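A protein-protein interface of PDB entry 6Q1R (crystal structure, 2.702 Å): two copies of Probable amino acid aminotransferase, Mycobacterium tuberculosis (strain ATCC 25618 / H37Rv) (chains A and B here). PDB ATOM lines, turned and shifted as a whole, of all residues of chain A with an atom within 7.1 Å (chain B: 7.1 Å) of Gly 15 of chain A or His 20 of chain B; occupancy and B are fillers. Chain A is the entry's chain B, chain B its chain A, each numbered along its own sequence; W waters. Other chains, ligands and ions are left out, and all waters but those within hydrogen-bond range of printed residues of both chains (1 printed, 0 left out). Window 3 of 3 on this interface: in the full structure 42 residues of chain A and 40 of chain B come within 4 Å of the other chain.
Water W1 bridges O of Pro 14 of chain A and NH2 of Arg 99 of chain B.
Among the printed residues, pairs that only touch across the chains: Pro 17 of chain A with Leu 19 of chain B (3.4 Å), Leu 19 of chain A with Pro 17 of chain B (3.5 Å), Val 4 of chain A with Ala 21 of chain B (3.6 Å), Leu 19 of chain A with Ala 26 of chain B (3.6 Å), Met 110 of chain A with Ala 21 of chain B (3.6 Å), Pro 17 of chain A with Pro 17 of chain B (3.7 Å), Leu 18 of chain A with Pro 17 of chain B (3.7 Å), Pro 17 of chain A with Leu 18 of chain B (3.7 Å), Leu 19 of chain A with His 20 of chain B (3.8 Å) and Met 110 of chain A with Asp 22 of chain B (3.9 Å).
Printed residues of chain B within 4 Å of Val 4 of chain A: Ala 21 (3.6 Å). Gly 15 of chain A touches just one residue of chain B: His 20. Of the printed residues of chain A, Asp 22 of chain B touches Met 110. Val 27 of chain B touches none of the printed residues of chain A. The nearest printed residue of chain A that does not touch His 20 of chain B is Pro 17 of chain A (4.1 Å). The nearest printed residue of chain A that does not touch Leu 18 of chain B is Leu 18 of chain A (5.6 Å).
Pro 17 of chain B touches its own counterpart, Pro 17 of chain A. Pro 17 of chain A touches Leu 18 of chain B, and with the chains exchanged Leu 18 of chain A touches Pro 17 of chain B. Leu 18 of chain A touches Leu 19 of chain B, and with the chains exchanged Leu 19 of chain A touches Leu 18 of chain B. Leu 19 of chain B touches its own counterpart, Leu 19 of chain A. Positions printed for both chains: 17, 18 and 19.
The guanidinium group (NH1) of Arg 99 of chain B sits close to a ring nitrogen (NE2) of His 20 of chain B (3.3 Å). OD1 of Asp 22 of chain B is in salt-bridge range of NE of Arg 99 of chain B (2.9 Å). The backbone NH of Leu 12 of chain A is in hydrogen-bond range of the backbone carbonyl oxygen of Val 4 of chain A, 3.0 Å away.
O of Leu 19 of chain A lies within hydrogen-bond range of N of Leu 18 of chain B (3.0 Å). The backbone carbonyl oxygen (O) of Leu 19 of chain B is in hydrogen-bond range of the backbone NH (N) of Leu 18 of chain A, 3.0 Å away. The backbone NH (N) of Leu 19 of chain A lies within hydrogen-bond range of the backbone carbonyl oxygen (O) of Leu 19 of chain B, at 3.0 Å. A ring nitrogen (NE2) of His 20 of chain B sits at hydrogen-bond distance from the backbone carbonyl oxygen of Gly 15 of chain A, 3.3 Å away. O of Ala 21 of chain B is in hydrogen-bond range of OH of Tyr 108 of chain A, 2.9 Å away.
Hydrophobic or aromatic side chains of chain A that line the printed part of chain B: Val 4, Pro 17, Leu 19, Tyr 108 and Met 110. Among the printed residues, 15 pairs touch across the chains.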
ATOM      1  N   VAL A   4     -11.697  31.042  -5.599  1.00  0.00           N
ATOM      2  CA  VAL A   4     -13.044  30.773  -5.115  1.00  0.00           C
ATOM      3  C   VAL A   4     -13.867  32.047  -5.233  1.00  0.00           C
ATOM      4  O   VAL A   4     -13.397  33.132  -4.871  1.00  0.00           O
ATOM      5  CB  VAL A   4     -13.030  30.258  -3.664  1.00  0.00           C
ATOM      6  CG1 VAL A   4     -14.448  30.023  -3.169  1.00  0.00           C
ATOM      7  CG2 VAL A   4     -12.205  28.989  -3.571  1.00  0.00           C
ATOM      8  N   LEU A  12     -12.506  34.985  -2.743  1.00  0.00           N
ATOM      9  CA  LEU A  12     -11.960  34.573  -1.466  1.00  0.00           C
ATOM     10  C   LEU A  12     -10.445  34.718  -1.470  1.00  0.00           C
ATOM     11  O   LEU A  12      -9.788  34.559  -2.503  1.00  0.00           O
ATOM     12  CB  LEU A  12     -12.338  33.117  -1.184  1.00  0.00           C
ATOM     13  CG  LEU A  12     -12.105  32.523   0.206  1.00  0.00           C
ATOM     14  CD1 LEU A  12     -12.984  33.197   1.248  1.00  0.00           C
ATOM     15  CD2 LEU A  12     -12.328  31.013   0.186  1.00  0.00           C
ATOM     16  N   GLN A  13      -9.895  35.020  -0.296  1.00  0.00           N
ATOM     17  CA  GLN A  13      -8.452  35.032  -0.132  1.00  0.00           C
ATOM     18  C   GLN A  13      -7.910  33.628  -0.386  1.00  0.00           C
ATOM     19  O   GLN A  13      -8.588  32.634  -0.108  1.00  0.00           O
ATOM     20  CB  GLN A  13      -8.066  35.530   1.261  1.00  0.00           C
ATOM     21  CG  GLN A  13      -8.358  37.014   1.500  1.00  0.00           C
ATOM     22  CD  GLN A  13      -9.834  37.314   1.693  1.00  0.00           C
ATOM     23  OE1 GLN A  13     -10.645  36.409   1.902  1.00  0.00           O
ATOM     24  NE2 GLN A  13     -10.191  38.594   1.619  1.00  0.00           N
ATOM     25  N   PRO A  14      -6.698  33.515  -0.940  1.00  0.00           N
ATOM     26  CA  PRO A  14      -6.232  32.191  -1.386  1.00  0.00           C
ATOM     27  C   PRO A  14      -6.139  31.159  -0.273  1.00  0.00           C
ATOM     28  O   PRO A  14      -6.391  29.972  -0.522  1.00  0.00           O
ATOM     29  CB  PRO A  14      -4.853  32.494  -2.002  1.00  0.00           C
ATOM     30  CG  PRO A  14      -4.801  33.993  -2.168  1.00  0.00           C
ATOM     31  CD  PRO A  14      -5.668  34.554  -1.099  1.00  0.00           C
ATOM     32  N   GLY A  15      -5.780  31.568   0.946  1.00  0.00           N
ATOM     33  CA  GLY A  15      -5.605  30.648   2.054  1.00  0.00           C
ATOM     34  C   GLY A  15      -6.780  30.424   2.992  1.00  0.00           C
ATOM     35  O   GLY A  15      -6.697  29.544   3.852  1.00  0.00           O
ATOM     36  N   MET A  16      -7.879  31.162   2.848  1.00  0.00           N
ATOM     37  CA  MET A  16      -8.971  31.065   3.822  1.00  0.00           C
ATOM     38  C   MET A  16      -9.829  29.822   3.612  1.00  0.00           C
ATOM     39  O   MET A  16     -10.272  29.560   2.490  1.00  0.00           O
ATOM     40  CB  MET A  16      -9.866  32.305   3.766  1.00  0.00           C
ATOM     41  CG  MET A  16      -9.398  33.498   4.576  1.00  0.00           C
ATOM     42  SD  MET A  16      -9.363  33.042   6.322  1.00  0.00           S
ATOM     43  CE  MET A  16     -11.125  32.912   6.658  1.00  0.00           C
ATOM     44  N   PRO A  17     -10.075  29.042   4.666  1.00  0.00           N
ATOM     45  CA  PRO A  17     -11.042  27.943   4.574  1.00  0.00           C
ATOM     46  C   PRO A  17     -12.458  28.486   4.462  1.00  0.00           C
ATOM     47  O   PRO A  17     -12.801  29.504   5.068  1.00  0.00           O
ATOM     48  CB  PRO A  17     -10.839  27.181   5.889  1.00  0.00           C
ATOM     49  CG  PRO A  17     -10.304  28.208   6.825  1.00  0.00           C
ATOM     50  CD  PRO A  17      -9.425  29.091   5.985  1.00  0.00           C
ATOM     51  N   LEU A  18     -13.287  27.791   3.689  1.00  0.00           N
ATOM     52  CA  LEU A  18     -14.642  28.243   3.387  1.00  0.00           C
ATOM     53  C   LEU A  18     -15.737  27.404   4.028  1.00  0.00           C
ATOM     54  O   LEU A  18     -16.721  27.962   4.521  1.00  0.00           O
ATOM     55  CB  LEU A  18     -14.853  28.259   1.870  1.00  0.00           C
ATOM     56  CG  LEU A  18     -16.247  28.624   1.360  1.00  0.00           C
ATOM     57  CD1 LEU A  18     -16.506  30.114   1.531  1.00  0.00           C
ATOM     58  CD2 LEU A  18     -16.428  28.189  -0.096  1.00  0.00           C
ATOM     59  N   LEU A  19     -15.600  26.082   4.036  1.00  0.00           N
ATOM     60  CA  LEU A  19     -16.685  25.192   4.425  1.00  0.00           C
ATOM     61  C   LEU A  19     -16.638  24.859   5.910  1.00  0.00           C
ATOM     62  O   LEU A  19     -15.571  24.817   6.526  1.00  0.00           O
ATOM     63  CB  LEU A  19     -16.633  23.902   3.608  1.00  0.00           C
ATOM     64  CG  LEU A  19     -16.606  24.149   2.103  1.00  0.00           C
ATOM     65  CD1 LEU A  19     -16.357  22.851   1.379  1.00  0.00           C
ATOM     66  CD2 LEU A  19     -17.887  24.811   1.626  1.00  0.00           C
ATOM     67  N   TYR A 108     -20.801  27.822  -4.342  1.00  0.00           N
ATOM     68  CA  TYR A 108     -19.653  28.615  -4.761  1.00  0.00           C
ATOM     69  C   TYR A 108     -19.122  28.042  -6.065  1.00  0.00           C
ATOM     70  O   TYR A 108     -19.375  26.884  -6.405  1.00  0.00           O
ATOM     71  CB  TYR A 108     -18.548  28.642  -3.698  1.00  0.00           C
ATOM     72  CG  TYR A 108     -17.968  27.288  -3.342  1.00  0.00           C
ATOM     73  CD1 TYR A 108     -18.556  26.494  -2.365  1.00  0.00           C
ATOM     74  CD2 TYR A 108     -16.823  26.811  -3.971  1.00  0.00           C
ATOM     75  CE1 TYR A 108     -18.024  25.258  -2.030  1.00  0.00           C
ATOM     76  CE2 TYR A 108     -16.282  25.574  -3.641  1.00  0.00           C
ATOM     77  CZ  TYR A 108     -16.888  24.804  -2.669  1.00  0.00           C
ATOM     78  OH  TYR A 108     -16.363  23.578  -2.329  1.00  0.00           O
ATOM     79  N   MET A 110     -15.510  27.554  -8.431  1.00  0.00           N
ATOM     80  CA  MET A 110     -14.085  27.396  -8.191  1.00  0.00           C
ATOM     81  C   MET A 110     -13.393  27.064  -9.500  1.00  0.00           C
ATOM     82  O   MET A 110     -13.827  26.162 -10.221  1.00  0.00           O
ATOM     83  CB  MET A 110     -13.818  26.293  -7.167  1.00  0.00           C
ATOM     84  CG  MET A 110     -12.351  25.980  -6.989  1.00  0.00           C
ATOM     85  SD  MET A 110     -12.067  24.875  -5.601  1.00  0.00           S
ATOM     86  CE  MET A 110     -13.110  23.485  -6.041  1.00  0.00           C
ATOM     87  N   PRO B  17     -15.239  28.166  10.057  1.00  0.00           N
ATOM     88  CA  PRO B  17     -14.976  27.250   8.942  1.00  0.00           C
ATOM     89  C   PRO B  17     -13.660  26.515   9.120  1.00  0.00           C
ATOM     90  O   PRO B  17     -12.654  27.086   9.546  1.00  0.00           O
ATOM     91  CB  PRO B  17     -14.930  28.177   7.721  1.00  0.00           C
ATOM     92  CG  PRO B  17     -15.601  29.442   8.166  1.00  0.00           C
ATOM     93  CD  PRO B  17     -15.294  29.569   9.617  1.00  0.00           C
ATOM     94  N   LEU B  18     -13.684  25.230   8.785  1.00  0.00           N
ATOM     95  CA  LEU B  18     -12.541  24.343   8.954  1.00  0.00           C
ATOM     96  C   LEU B  18     -11.979  23.859   7.628  1.00  0.00           C
ATOM     97  O   LEU B  18     -10.759  23.806   7.461  1.00  0.00           O
ATOM     98  CB  LEU B  18     -12.935  23.140   9.828  1.00  0.00           C
ATOM     99  CG  LEU B  18     -11.968  22.010  10.218  1.00  0.00           C
ATOM    100  CD1 LEU B  18     -12.577  21.220  11.352  1.00  0.00           C
ATOM    101  CD2 LEU B  18     -11.601  21.053   9.101  1.00  0.00           C
ATOM    102  N   LEU B  19     -12.847  23.504   6.684  1.00  0.00           N
ATOM    103  CA  LEU B  19     -12.448  22.853   5.446  1.00  0.00           C
ATOM    104  C   LEU B  19     -12.189  23.873   4.348  1.00  0.00           C
ATOM    105  O   LEU B  19     -12.823  24.930   4.287  1.00  0.00           O
ATOM    106  CB  LEU B  19     -13.533  21.879   4.986  1.00  0.00           C
ATOM    107  CG  LEU B  19     -13.982  20.791   5.961  1.00  0.00           C
ATOM    108  CD1 LEU B  19     -15.211  20.108   5.435  1.00  0.00           C
ATOM    109  CD2 LEU B  19     -12.878  19.768   6.124  1.00  0.00           C
ATOM    110  N   HIS B  20     -11.256  23.538   3.465  1.00  0.00           N
ATOM    111  CA  HIS B  20     -10.984  24.374   2.310  1.00  0.00           C
ATOM    112  C   HIS B  20     -11.957  24.058   1.178  1.00  0.00           C
ATOM    113  O   HIS B  20     -12.577  22.993   1.134  1.00  0.00           O
ATOM    114  CB  HIS B  20      -9.544  24.194   1.838  1.00  0.00           C
ATOM    115  CG  HIS B  20      -8.541  24.917   2.680  1.00  0.00           C
ATOM    116  ND1 HIS B  20      -7.993  24.373   3.820  1.00  0.00           N
ATOM    117  CD2 HIS B  20      -7.983  26.143   2.541  1.00  0.00           C
ATOM    118  CE1 HIS B  20      -7.143  25.235   4.351  1.00  0.00           C
ATOM    119  NE2 HIS B  20      -7.117  26.315   3.594  1.00  0.00           N
ATOM    120  N   ALA B  21     -12.092  25.014   0.259  1.00  0.00           N
ATOM    121  CA  ALA B  21     -13.028  24.851  -0.844  1.00  0.00           C
ATOM    122  C   ALA B  21     -12.654  23.708  -1.778  1.00  0.00           C
ATOM    123  O   ALA B  21     -13.528  23.201  -2.487  1.00  0.00           O
ATOM    124  CB  ALA B  21     -13.130  26.147  -1.643  1.00  0.00           C
ATOM    125  N   ASP B  22     -11.389  23.286  -1.794  1.00  0.00           N
ATOM    126  CA  ASP B  22     -10.940  22.206  -2.668  1.00  0.00           C
ATOM    127  C   ASP B  22     -10.658  20.916  -1.905  1.00  0.00           C
ATOM    128  O   ASP B  22      -9.921  20.058  -2.396  1.00  0.00           O
ATOM    129  CB  ASP B  22      -9.710  22.642  -3.468  1.00  0.00           C
ATOM    130  CG  ASP B  22      -8.520  22.987  -2.588  1.00  0.00           C
ATOM    131  OD1 ASP B  22      -8.695  23.110  -1.358  1.00  0.00           O
ATOM    132  OD2 ASP B  22      -7.407  23.147  -3.136  1.00  0.00           O
ATOM    133  N   ASP B  23     -11.228  20.762  -0.717  1.00  0.00           N
ATOM    134  CA  ASP B  23     -11.071  19.525   0.031  1.00  0.00           C
ATOM    135  C   ASP B  23     -11.890  18.422  -0.627  1.00  0.00           C
ATOM    136  O   ASP B  23     -13.086  18.591  -0.890  1.00  0.00           O
ATOM    137  CB  ASP B  23     -11.504  19.731   1.479  1.00  0.00           C
ATOM    138  CG  ASP B  23     -11.078  18.597   2.384  1.00  0.00           C
ATOM    139  OD1 ASP B  23     -11.448  17.435   2.107  1.00  0.00           O
ATOM    140  OD2 ASP B  23     -10.358  18.870   3.369  1.00  0.00           O
ATOM    141  N   LEU B  24     -11.245  17.281  -0.881  1.00  0.00           N
ATOM    142  CA  LEU B  24     -11.869  16.193  -1.625  1.00  0.00           C
ATOM    143  C   LEU B  24     -13.069  15.582  -0.909  1.00  0.00           C
ATOM    144  O   LEU B  24     -13.816  14.827  -1.540  1.00  0.00           O
ATOM    145  CB  LEU B  24     -10.832  15.110  -1.923  1.00  0.00           C
ATOM    146  CG  LEU B  24      -9.785  15.471  -2.981  1.00  0.00           C
ATOM    147  CD1 LEU B  24      -8.667  14.450  -2.981  1.00  0.00           C
ATOM    148  CD2 LEU B  24     -10.409  15.580  -4.358  1.00  0.00           C
ATOM    149  N   ALA B  26     -15.616  17.326   0.192  1.00  0.00           N
ATOM    150  CA  ALA B  26     -16.741  18.076  -0.344  1.00  0.00           C
ATOM    151  C   ALA B  26     -16.745  18.136  -1.862  1.00  0.00           C
ATOM    152  O   ALA B  26     -17.820  18.194  -2.463  1.00  0.00           O
ATOM    153  CB  ALA B  26     -16.743  19.501   0.214  1.00  0.00           C
ATOM    154  N   VAL B  27     -15.572  18.111  -2.493  1.00  0.00           N
ATOM    155  CA  VAL B  27     -15.510  18.218  -3.945  1.00  0.00           C
ATOM    156  C   VAL B  27     -15.889  16.900  -4.605  1.00  0.00           C
ATOM    157  O   VAL B  27     -16.560  16.886  -5.643  1.00  0.00           O
ATOM    158  CB  VAL B  27     -14.110  18.695  -4.376  1.00  0.00           C
ATOM    159  CG1 VAL B  27     -13.937  18.596  -5.882  1.00  0.00           C
ATOM    160  CG2 VAL B  27     -13.895  20.123  -3.933  1.00  0.00           C
ATOM    161  N   ARG B  99      -6.855  17.870   0.512  1.00  0.00           N
ATOM    162  CA  ARG B  99      -7.026  18.829  -0.568  1.00  0.00           C
ATOM    163  C   ARG B  99      -6.460  18.272  -1.873  1.00  0.00           C
ATOM    164  O   ARG B  99      -5.728  17.279  -1.893  1.00  0.00           O
ATOM    165  CB  ARG B  99      -6.361  20.160  -0.215  1.00  0.00           C
ATOM    166  CG  ARG B  99      -6.884  20.781   1.064  1.00  0.00           C
ATOM    167  CD  ARG B  99      -6.268  22.146   1.313  1.00  0.00           C
ATOM    168  NE  ARG B  99      -6.220  22.965   0.105  1.00  0.00           N
ATOM    169  CZ  ARG B  99      -5.819  24.234   0.082  1.00  0.00           C
ATOM    170  NH1 ARG B  99      -5.427  24.828   1.202  1.00  0.00           N
ATOM    171  NH2 ARG B  99      -5.808  24.909  -1.061  1.00  0.00           N
ATOM    172  N   THR B 106      -7.323  14.864   5.396  1.00  0.00           N
ATOM    173  CA  THR B 106      -8.153  15.601   6.345  1.00  0.00           C
ATOM    174  C   THR B 106      -8.745  14.642   7.369  1.00  0.00           C
ATOM    175  O   THR B 106      -9.369  13.644   6.998  1.00  0.00           O
ATOM    176  CB  THR B 106      -9.279  16.338   5.621  1.00  0.00           C
ATOM    177  OG1 THR B 106      -8.730  17.263   4.676  1.00  0.00           O
ATOM    178  CG2 THR B 106     -10.152  17.083   6.606  1.00  0.00           C
HETATM  179  O   HOH W   1      -4.202  27.895  -1.365  1.00  0.00           O
